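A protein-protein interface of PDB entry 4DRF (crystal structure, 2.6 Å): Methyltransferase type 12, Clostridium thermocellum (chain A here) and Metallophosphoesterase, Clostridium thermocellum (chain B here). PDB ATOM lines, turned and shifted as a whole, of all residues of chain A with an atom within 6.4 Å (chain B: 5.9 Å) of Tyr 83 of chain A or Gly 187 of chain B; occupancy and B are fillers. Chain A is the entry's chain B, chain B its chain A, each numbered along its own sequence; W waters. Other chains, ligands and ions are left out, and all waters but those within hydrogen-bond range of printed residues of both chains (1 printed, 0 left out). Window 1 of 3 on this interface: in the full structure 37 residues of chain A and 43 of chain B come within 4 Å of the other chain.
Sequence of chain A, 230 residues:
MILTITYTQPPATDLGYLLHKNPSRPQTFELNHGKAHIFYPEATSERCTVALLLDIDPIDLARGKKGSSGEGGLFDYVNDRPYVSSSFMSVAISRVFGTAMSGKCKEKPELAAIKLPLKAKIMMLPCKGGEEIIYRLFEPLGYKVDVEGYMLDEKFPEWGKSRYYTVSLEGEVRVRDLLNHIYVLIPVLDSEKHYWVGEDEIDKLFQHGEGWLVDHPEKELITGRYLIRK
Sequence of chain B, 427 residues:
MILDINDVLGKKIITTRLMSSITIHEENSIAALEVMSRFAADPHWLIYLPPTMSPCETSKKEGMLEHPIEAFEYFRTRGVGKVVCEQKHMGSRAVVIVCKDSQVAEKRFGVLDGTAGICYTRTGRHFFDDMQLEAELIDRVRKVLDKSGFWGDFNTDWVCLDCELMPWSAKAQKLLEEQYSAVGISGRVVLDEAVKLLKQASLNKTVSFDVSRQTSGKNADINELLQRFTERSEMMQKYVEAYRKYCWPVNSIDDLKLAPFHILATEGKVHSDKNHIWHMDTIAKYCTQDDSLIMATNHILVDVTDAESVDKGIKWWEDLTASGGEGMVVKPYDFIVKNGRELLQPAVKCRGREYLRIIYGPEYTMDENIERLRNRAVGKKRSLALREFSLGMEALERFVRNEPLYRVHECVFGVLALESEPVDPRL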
ATOM      1  N   MET A   1     -24.909   1.272  15.660  1.00  0.00           N
ATOM      2  CA  MET A   1     -23.991   1.746  16.687  1.00  0.00           C
ATOM      3  C   MET A   1     -24.692   1.939  18.032  1.00  0.00           C
ATOM      4  O   MET A   1     -24.075   2.372  19.013  1.00  0.00           O
ATOM      5  CB  MET A   1     -23.319   3.048  16.268  1.00  0.00           C
ATOM      6  CG  MET A   1     -24.075   4.334  16.587  1.00  0.00           C
ATOM      7  SD  MET A   1     -22.978   5.766  16.467  1.00  0.00           S
ATOM      8  CE  MET A   1     -21.574   4.906  17.056  1.00  0.00           C
ATOM      9  N   ILE A   2     -25.987   1.637  18.068  1.00  0.00           N
ATOM     10  CA  ILE A   2     -26.755   1.793  19.299  1.00  0.00           C
ATOM     11  C   ILE A   2     -27.520   0.532  19.730  1.00  0.00           C
ATOM     12  O   ILE A   2     -28.218  -0.098  18.932  1.00  0.00           O
ATOM     13  CB  ILE A   2     -27.716   2.980  19.219  1.00  0.00           C
ATOM     14  CG1 ILE A   2     -26.959   4.228  18.807  1.00  0.00           C
ATOM     15  CG2 ILE A   2     -28.373   3.233  20.566  1.00  0.00           C
ATOM     16  CD1 ILE A   2     -27.847   5.378  18.516  1.00  0.00           C
ATOM     17  N   ILE A  56     -16.597   5.346  18.205  1.00  0.00           N
ATOM     18  CA  ILE A  56     -15.424   4.820  17.515  1.00  0.00           C
ATOM     19  C   ILE A  56     -14.616   5.945  16.824  1.00  0.00           C
ATOM     20  O   ILE A  56     -15.175   6.858  16.208  1.00  0.00           O
ATOM     21  CB  ILE A  56     -15.820   3.756  16.447  1.00  0.00           C
ATOM     22  CG1 ILE A  56     -16.782   2.688  17.010  1.00  0.00           C
ATOM     23  CG2 ILE A  56     -14.575   3.152  15.789  1.00  0.00           C
ATOM     24  CD1 ILE A  56     -16.233   1.854  18.164  1.00  0.00           C
ATOM     25  N   PRO A  58     -12.358   7.233  14.007  1.00  0.00           N
ATOM     26  CA  PRO A  58     -12.076   6.837  12.618  1.00  0.00           C
ATOM     27  C   PRO A  58     -10.577   6.766  12.330  1.00  0.00           C
ATOM     28  O   PRO A  58     -10.147   5.865  11.613  1.00  0.00           O
ATOM     29  CB  PRO A  58     -12.736   7.938  11.796  1.00  0.00           C
ATOM     30  CG  PRO A  58     -12.789   9.124  12.727  1.00  0.00           C
ATOM     31  CD  PRO A  58     -12.935   8.584  14.109  1.00  0.00           C
ATOM     32  N   ASN A  79     -15.051   4.526   5.959  1.00  0.00           N
ATOM     33  CA  ASN A  79     -15.857   3.302   6.098  1.00  0.00           C
ATOM     34  C   ASN A  79     -17.000   3.422   7.088  1.00  0.00           C
ATOM     35  O   ASN A  79     -17.067   4.373   7.877  1.00  0.00           O
ATOM     36  CB  ASN A  79     -14.983   2.098   6.481  1.00  0.00           C
ATOM     37  CG  ASN A  79     -14.054   2.403   7.612  1.00  0.00           C
ATOM     38  OD1 ASN A  79     -14.488   2.639   8.732  1.00  0.00           O
ATOM     39  ND2 ASN A  79     -12.764   2.406   7.332  1.00  0.00           N
ATOM     40  N   ASP A  80     -17.886   2.434   7.058  1.00  0.00           N
ATOM     41  CA  ASP A  80     -19.051   2.435   7.938  1.00  0.00           C
ATOM     42  C   ASP A  80     -18.795   1.945   9.373  1.00  0.00           C
ATOM     43  O   ASP A  80     -19.733   1.820  10.156  1.00  0.00           O
ATOM     44  CB  ASP A  80     -20.202   1.670   7.305  1.00  0.00           C
ATOM     45  CG  ASP A  80     -19.975   0.167   7.257  1.00  0.00           C
ATOM     46  OD1 ASP A  80     -18.913  -0.344   7.704  1.00  0.00           O
ATOM     47  OD2 ASP A  80     -20.885  -0.506   6.739  1.00  0.00           O
ATOM     48  N   ARG A  81     -17.535   1.704   9.724  1.00  0.00           N
ATOM     49  CA  ARG A  81     -17.208   1.130  11.036  1.00  0.00           C
ATOM     50  C   ARG A  81     -17.709   1.903  12.250  1.00  0.00           C
ATOM     51  O   ARG A  81     -18.224   1.279  13.187  1.00  0.00           O
ATOM     52  CB  ARG A  81     -15.709   0.790  11.173  1.00  0.00           C
ATOM     53  CG  ARG A  81     -15.293  -0.593  10.598  1.00  0.00           C
ATOM     54  CD  ARG A  81     -16.469  -1.294   9.858  1.00  0.00           C
ATOM     55  NE  ARG A  81     -16.662  -2.680  10.280  1.00  0.00           N
ATOM     56  CZ  ARG A  81     -17.665  -3.462   9.884  1.00  0.00           C
ATOM     57  NH1 ARG A  81     -18.587  -3.009   9.051  1.00  0.00           N
ATOM     58  NH2 ARG A  81     -17.744  -4.711  10.326  1.00  0.00           N
ATOM     59  N   PRO A  82     -17.585   3.249  12.243  1.00  0.00           N
ATOM     60  CA  PRO A  82     -17.959   3.948  13.481  1.00  0.00           C
ATOM     61  C   PRO A  82     -19.463   4.062  13.690  1.00  0.00           C
ATOM     62  O   PRO A  82     -19.859   4.625  14.711  1.00  0.00           O
ATOM     63  CB  PRO A  82     -17.356   5.361  13.302  1.00  0.00           C
ATOM     64  CG  PRO A  82     -16.426   5.246  12.147  1.00  0.00           C
ATOM     65  CD  PRO A  82     -17.022   4.188  11.265  1.00  0.00           C
ATOM     66  N   TYR A  83     -20.263   3.524  12.769  1.00  0.00           N
ATOM     67  CA  TYR A  83     -21.701   3.794  12.727  1.00  0.00           C
ATOM     68  C   TYR A  83     -22.528   2.516  12.679  1.00  0.00           C
ATOM     69  O   TYR A  83     -23.742   2.580  12.536  1.00  0.00           O
ATOM     70  CB  TYR A  83     -22.053   4.666  11.483  1.00  0.00           C
ATOM     71  CG  TYR A  83     -21.102   5.817  11.254  1.00  0.00           C
ATOM     72  CD1 TYR A  83     -21.035   6.860  12.157  1.00  0.00           C
ATOM     73  CD2 TYR A  83     -20.253   5.849  10.152  1.00  0.00           C
ATOM     74  CE1 TYR A  83     -20.168   7.898  11.989  1.00  0.00           C
ATOM     75  CE2 TYR A  83     -19.364   6.885   9.968  1.00  0.00           C
ATOM     76  CZ  TYR A  83     -19.327   7.923  10.890  1.00  0.00           C
ATOM     77  OH  TYR A  83     -18.461   8.997  10.751  1.00  0.00           O
ATOM     78  N   VAL A  84     -21.876   1.366  12.732  1.00  0.00           N
ATOM     79  CA  VAL A  84     -22.590   0.090  12.680  1.00  0.00           C
ATOM     80  C   VAL A  84     -22.462  -0.700  13.988  1.00  0.00           C
ATOM     81  O   VAL A  84     -21.521  -0.504  14.762  1.00  0.00           O
ATOM     82  CB  VAL A  84     -22.092  -0.801  11.519  1.00  0.00           C
ATOM     83  CG1 VAL A  84     -22.130  -0.060  10.209  1.00  0.00           C
ATOM     84  CG2 VAL A  84     -20.712  -1.296  11.799  1.00  0.00           C
ATOM     85  N   SER A  85     -23.404  -1.597  14.234  1.00  0.00           N
ATOM     86  CA  SER A  85     -23.285  -2.510  15.381  1.00  0.00           C
ATOM     87  C   SER A  85     -22.406  -3.711  15.002  1.00  0.00           C
ATOM     88  O   SER A  85     -22.885  -4.791  14.686  1.00  0.00           O
ATOM     89  CB  SER A  85     -24.664  -2.929  15.898  1.00  0.00           C
ATOM     90  OG  SER A  85     -25.373  -1.800  16.360  1.00  0.00           O
ATOM     91  N   MET A 123     -29.209  -1.189  16.403  1.00  0.00           N
ATOM     92  CA  MET A 123     -29.214  -0.420  15.155  1.00  0.00           C
ATOM     93  C   MET A 123     -28.079  -0.761  14.234  1.00  0.00           C
ATOM     94  O   MET A 123     -26.954  -1.023  14.689  1.00  0.00           O
ATOM     95  CB  MET A 123     -29.246   1.071  15.421  1.00  0.00           C
ATOM     96  CG  MET A 123     -30.563   1.476  16.021  1.00  0.00           C
ATOM     97  SD  MET A 123     -30.734   3.223  16.301  1.00  0.00           S
ATOM     98  CE  MET A 123     -31.066   3.784  14.656  1.00  0.00           C
ATOM     99  N   MET A 124     -28.407  -0.796  12.943  1.00  0.00           N
ATOM    100  CA  MET A 124     -27.394  -0.755  11.885  1.00  0.00           C
ATOM    101  C   MET A 124     -26.484  -1.946  11.962  1.00  0.00           C
ATOM    102  O   MET A 124     -25.249  -1.825  12.085  1.00  0.00           O
ATOM    103  CB  MET A 124     -26.568   0.534  11.949  1.00  0.00           C
ATOM    104  CG  MET A 124     -26.772   1.410  10.744  1.00  0.00           C
ATOM    105  SD  MET A 124     -28.510   1.626  10.429  1.00  0.00           S
ATOM    106  CE  MET A 124     -28.484   2.286   8.772  1.00  0.00           C
ATOM    107  N   ALA B 182     -23.269   4.147   1.569  1.00  0.00           N
ATOM    108  CA  ALA B 182     -23.320   3.164   2.656  1.00  0.00           C
ATOM    109  C   ALA B 182     -22.944   3.822   3.984  1.00  0.00           C
ATOM    110  O   ALA B 182     -23.698   3.781   4.949  1.00  0.00           O
ATOM    111  CB  ALA B 182     -22.412   1.991   2.351  1.00  0.00           C
ATOM    112  N   VAL B 183     -21.779   4.453   3.997  1.00  0.00           N
ATOM    113  CA  VAL B 183     -21.352   5.321   5.089  1.00  0.00           C
ATOM    114  C   VAL B 183     -22.352   6.421   5.406  1.00  0.00           C
ATOM    115  O   VAL B 183     -22.564   6.751   6.564  1.00  0.00           O
ATOM    116  CB  VAL B 183     -19.990   5.966   4.761  1.00  0.00           C
ATOM    117  CG1 VAL B 183     -19.573   6.979   5.836  1.00  0.00           C
ATOM    118  CG2 VAL B 183     -18.937   4.889   4.563  1.00  0.00           C
ATOM    119  N   GLY B 184     -22.965   6.983   4.365  1.00  0.00           N
ATOM    120  CA  GLY B 184     -23.905   8.080   4.503  1.00  0.00           C
ATOM    121  C   GLY B 184     -25.229   7.721   5.189  1.00  0.00           C
ATOM    122  O   GLY B 184     -25.679   8.442   6.080  1.00  0.00           O
ATOM    123  N   ILE B 185     -25.865   6.624   4.766  1.00  0.00           N
ATOM    124  CA  ILE B 185     -27.075   6.141   5.413  1.00  0.00           C
ATOM    125  C   ILE B 185     -26.837   5.640   6.860  1.00  0.00           C
ATOM    126  O   ILE B 185     -27.610   5.948   7.772  1.00  0.00           O
ATOM    127  CB  ILE B 185     -27.785   5.051   4.595  1.00  0.00           C
ATOM    128  CG1 ILE B 185     -29.131   4.747   5.244  1.00  0.00           C
ATOM    129  CG2 ILE B 185     -26.921   3.787   4.449  1.00  0.00           C
ATOM    130  CD1 ILE B 185     -29.967   5.978   5.430  1.00  0.00           C
ATOM    131  N   SER B 186     -25.761   4.890   7.076  1.00  0.00           N
ATOM    132  CA  SER B 186     -25.523   4.320   8.385  1.00  0.00           C
ATOM    133  C   SER B 186     -25.203   5.430   9.370  1.00  0.00           C
ATOM    134  O   SER B 186     -25.674   5.428  10.509  1.00  0.00           O
ATOM    135  CB  SER B 186     -24.402   3.272   8.324  1.00  0.00           C
ATOM    136  OG  SER B 186     -23.167   3.852   7.926  1.00  0.00           O
ATOM    137  N   GLY B 187     -24.398   6.381   8.917  1.00  0.00           N
ATOM    138  CA  GLY B 187     -23.992   7.514   9.732  1.00  0.00           C
ATOM    139  C   GLY B 187     -25.123   8.483  10.045  1.00  0.00           C
ATOM    140  O   GLY B 187     -25.269   8.925  11.186  1.00  0.00           O
ATOM    141  N   ARG B 188     -25.934   8.825   9.049  1.00  0.00           N
ATOM    142  CA  ARG B 188     -27.074   9.708   9.334  1.00  0.00           C
ATOM    143  C   ARG B 188     -28.055   9.133  10.350  1.00  0.00           C
ATOM    144  O   ARG B 188     -28.396   9.808  11.307  1.00  0.00           O
ATOM    145  CB  ARG B 188     -27.801  10.153   8.068  1.00  0.00           C
ATOM    146  CG  ARG B 188     -27.081  11.314   7.372  1.00  0.00           C
ATOM    147  CD  ARG B 188     -27.754  11.664   6.071  1.00  0.00           C
ATOM    148  NE  ARG B 188     -27.812  10.517   5.163  1.00  0.00           N
ATOM    149  CZ  ARG B 188     -28.898  10.187   4.475  1.00  0.00           C
ATOM    150  NH1 ARG B 188     -30.014  10.893   4.601  1.00  0.00           N
ATOM    151  NH2 ARG B 188     -28.878   9.150   3.665  1.00  0.00           N
ATOM    152  N   VAL B 189     -28.477   7.887  10.149  1.00  0.00           N
ATOM    153  CA  VAL B 189     -29.466   7.247  11.010  1.00  0.00           C
ATOM    154  C   VAL B 189     -29.044   7.135  12.483  1.00  0.00           C
ATOM    155  O   VAL B 189     -29.773   7.561  13.385  1.00  0.00           O
ATOM    156  CB  VAL B 189     -29.832   5.851  10.480  1.00  0.00           C
ATOM    157  CG1 VAL B 189     -30.761   5.139  11.462  1.00  0.00           C
ATOM    158  CG2 VAL B 189     -30.499   5.980   9.128  1.00  0.00           C
ATOM    159  N   VAL B 190     -27.873   6.553  12.721  1.00  0.00           N
ATOM    160  CA  VAL B 190     -27.401   6.364  14.077  1.00  0.00           C
ATOM    161  C   VAL B 190     -27.049   7.674  14.790  1.00  0.00           C
ATOM    162  O   VAL B 190     -27.268   7.807  16.000  1.00  0.00           O
ATOM    163  CB  VAL B 190     -26.212   5.393  14.157  1.00  0.00           C
ATOM    164  CG1 VAL B 190     -26.584   4.087  13.555  1.00  0.00           C
ATOM    165  CG2 VAL B 190     -24.956   5.980  13.485  1.00  0.00           C
ATOM    166  N   LEU B 191     -26.513   8.641  14.054  1.00  0.00           N
ATOM    167  CA  LEU B 191     -26.144   9.910  14.667  1.00  0.00           C
ATOM    168  C   LEU B 191     -27.378  10.744  14.989  1.00  0.00           C
ATOM    169  O   LEU B 191     -27.374  11.532  15.932  1.00  0.00           O
ATOM    170  CB  LEU B 191     -25.164  10.692  13.785  1.00  0.00           C
ATOM    171  CG  LEU B 191     -23.782  10.057  13.681  1.00  0.00           C
ATOM    172  CD1 LEU B 191     -22.984  10.771  12.657  1.00  0.00           C
ATOM    173  CD2 LEU B 191     -23.076  10.075  15.034  1.00  0.00           C
ATOM    174  N   ASP B 192     -28.430  10.572  14.201  1.00  0.00           N
ATOM    175  CA  ASP B 192     -29.696  11.245  14.482  1.00  0.00           C
ATOM    176  C   ASP B 192     -30.373  10.567  15.664  1.00  0.00           C
ATOM    177  O   ASP B 192     -30.946  11.222  16.532  1.00  0.00           O
ATOM    178  CB  ASP B 192     -30.629  11.235  13.267  1.00  0.00           C
ATOM    179  CG  ASP B 192     -30.214  12.240  12.194  1.00  0.00           C
ATOM    180  OD1 ASP B 192     -29.153  12.889  12.349  1.00  0.00           O
ATOM    181  OD2 ASP B 192     -30.952  12.367  11.189  1.00  0.00           O
ATOM    182  N   ARG B 232     -21.133  15.715  15.416  1.00  0.00           N
ATOM    183  CA  ARG B 232     -20.931  14.579  14.529  1.00  0.00           C
ATOM    184  C   ARG B 232     -22.051  14.461  13.501  1.00  0.00           C
ATOM    185  O   ARG B 232     -21.800  14.263  12.315  1.00  0.00           O
ATOM    186  CB  ARG B 232     -20.790  13.283  15.321  1.00  0.00           C
ATOM    187  CG  ARG B 232     -19.654  13.299  16.312  1.00  0.00           C
ATOM    188  CD  ARG B 232     -19.427  11.921  16.912  1.00  0.00           C
ATOM    189  NE  ARG B 232     -19.170  10.911  15.886  1.00  0.00           N
ATOM    190  CZ  ARG B 232     -19.078   9.598  16.111  1.00  0.00           C
ATOM    191  NH1 ARG B 232     -19.239   9.094  17.332  1.00  0.00           N
ATOM    192  NH2 ARG B 232     -18.838   8.775  15.104  1.00  0.00           N
ATOM    193  N   MET B 236     -21.807  14.801   9.287  1.00  0.00           N
ATOM    194  CA  MET B 236     -22.320  13.695   8.504  1.00  0.00           C
ATOM    195  C   MET B 236     -23.389  14.157   7.501  1.00  0.00           C
ATOM    196  O   MET B 236     -23.556  13.552   6.439  1.00  0.00           O
ATOM    197  CB  MET B 236     -22.857  12.618   9.468  1.00  0.00           C
ATOM    198  CG  MET B 236     -23.579  11.445   8.833  1.00  0.00           C
ATOM    199  SD  MET B 236     -22.491  10.421   7.821  1.00  0.00           S
ATOM    200  CE  MET B 236     -21.338   9.838   9.039  1.00  0.00           C
ATOM    201  N   PRO B 362     -16.180  11.878   6.585  1.00  0.00           N
ATOM    202  CA  PRO B 362     -17.283  12.725   7.070  1.00  0.00           C
ATOM    203  C   PRO B 362     -16.896  13.656   8.211  1.00  0.00           C
ATOM    204  O   PRO B 362     -17.317  14.818   8.227  1.00  0.00           O
ATOM    205  CB  PRO B 362     -18.314  11.695   7.589  1.00  0.00           C
ATOM    206  CG  PRO B 362     -17.590  10.368   7.600  1.00  0.00           C
ATOM    207  CD  PRO B 362     -16.593  10.470   6.494  1.00  0.00           C
ATOM    208  N   GLU B 363     -16.104  13.143   9.152  1.00  0.00           N
ATOM    209  CA  GLU B 363     -15.833  13.843  10.407  1.00  0.00           C
ATOM    210  C   GLU B 363     -14.414  14.357  10.518  1.00  0.00           C
ATOM    211  O   GLU B 363     -13.886  14.482  11.630  1.00  0.00           O
ATOM    212  CB  GLU B 363     -16.083  12.904  11.581  1.00  0.00           C
ATOM    213  CG  GLU B 363     -17.472  12.321  11.606  1.00  0.00           C
ATOM    214  CD  GLU B 363     -17.688  11.444  12.784  1.00  0.00           C
ATOM    215  OE1 GLU B 363     -17.060  11.702  13.836  1.00  0.00           O
ATOM    216  OE2 GLU B 363     -18.468  10.490  12.641  1.00  0.00           O
HETATM  217  O   HOH W   1     -18.906   5.930  16.665  1.00  0.00           O
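Water W1 lies within hydrogen-bond range of the backbone carbonyl oxygen of Pro 82 of chain A, the backbone NH of Ile 56 of chain A and the guanidinium group of Arg 232 of chain B.
Of chain B, only Ser 186, Gly 187, Val 190, Arg 232, Met 236, Pro 362 and Glu 363 come within 4 Å of Tyr 83 of chain A. Of the printed residues of chain B, Met 123 of chain A touches Val 189. Printed residues of chain A within 4 Å of Val 183 of chain B: Asn 79 (3.5 Å) and Asp 80 (3.7 Å). Gly 187 of chain B touches one residue of chain A. The nearest printed residue of chain B that does not touch Asn 79 of chain A is Pro 362 of chain B (6.0 Å).
The side-chain carboxylate of Glu 363 of chain B is in hydrogen-bond range of the side-chain hydroxyl of Tyr 83 of chain A (2.4 Å).
Hydrophobic or aromatic side chains of chain B within 4 Å of the printed part of chain A: Val 183, Val 189, Val 190, Met 236 and Pro 362. Of the 13 printed residues of chain A, 7 touch a printed residue of chain B. Printed residues of chain A that touch a printed residue of chain B: Met 1, Ile 2, Asn 79, Asp 80, Tyr 83, Met 123 and Met 124. Hydrophobic or aromatic side chains of chain A within 4 Å of the printed part of chain B: Met 1, Ile 2, Tyr 83, Met 123 and Met 124. Among the printed residues, no Asp or Glu carboxylate lies within 4 Å of a Lys or Arg side-chain nitrogen of the other chain.
The backbone carbonyl oxygen of Ala 182 of chain B lies within hydrogen-bond range of the side-chain hydroxyl of Ser 186 of chain B, 3.0 Å away. N of Met 1 of chain A sits at hydrogen-bond distance from OG of Ser 85 of chain A. The backbone NH (N) of Met 1 of chain A lies within hydrogen-bond range of the backbone carbonyl oxygen (O) of Met 123 of chain A (3.2 Å). The backbone carbonyl oxygen (O) of Ile 2 of chain A is in hydrogen-bond range of the backbone NH (N) of Met 123 of chain A (2.9 Å). OD1 of Asp 80 of chain A is in salt-bridge range of NH1 of Arg 81 of chain A (3.0 Å). The backbone carbonyl oxygen of Met 123 of chain A sits at hydrogen-bond distance from the side-chain hydroxyl of Ser 85 of chain A (2.4 Å).
Among the printed residues, merely in contact across the chains: Tyr 83 of chain A with Met 236 of chain B (3.3 Å), Tyr 83 of chain A with Val 190 of chain B (3.4 Å), Met 1 of chain A with Val 190 of chain B (3.4 Å), Met 123 of chain A with Val 189 of chain B (3.5 Å), Tyr 83 of chain A with Arg 232 of chain B (3.5 Å), Asn 79 of chain A with Val 183 of chain B (3.5 Å), Ile 2 of chain A with Val 190 of chain B (3.5 Å), Tyr 83 of chain A with Pro 362 of chain B (3.5 Å), Met 124 of chain A with Ser 186 of chain B (3.6 Å), Asp 80 of chain A with Val 183 of chain B (3.7 Å), Tyr 83 of chain A with Gly 187 of chain B (3.7 Å), Asp 80 of chain A with Ser 186 of chain B (3.7 Å), Tyr 83 of chain A with Ser 186 of chain B (3.8 Å), Met 124 of chain A with Val 190 of chain B (3.9 Å) and Met 124 of chain A with Ile 185 of chain B (3.9 Å).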
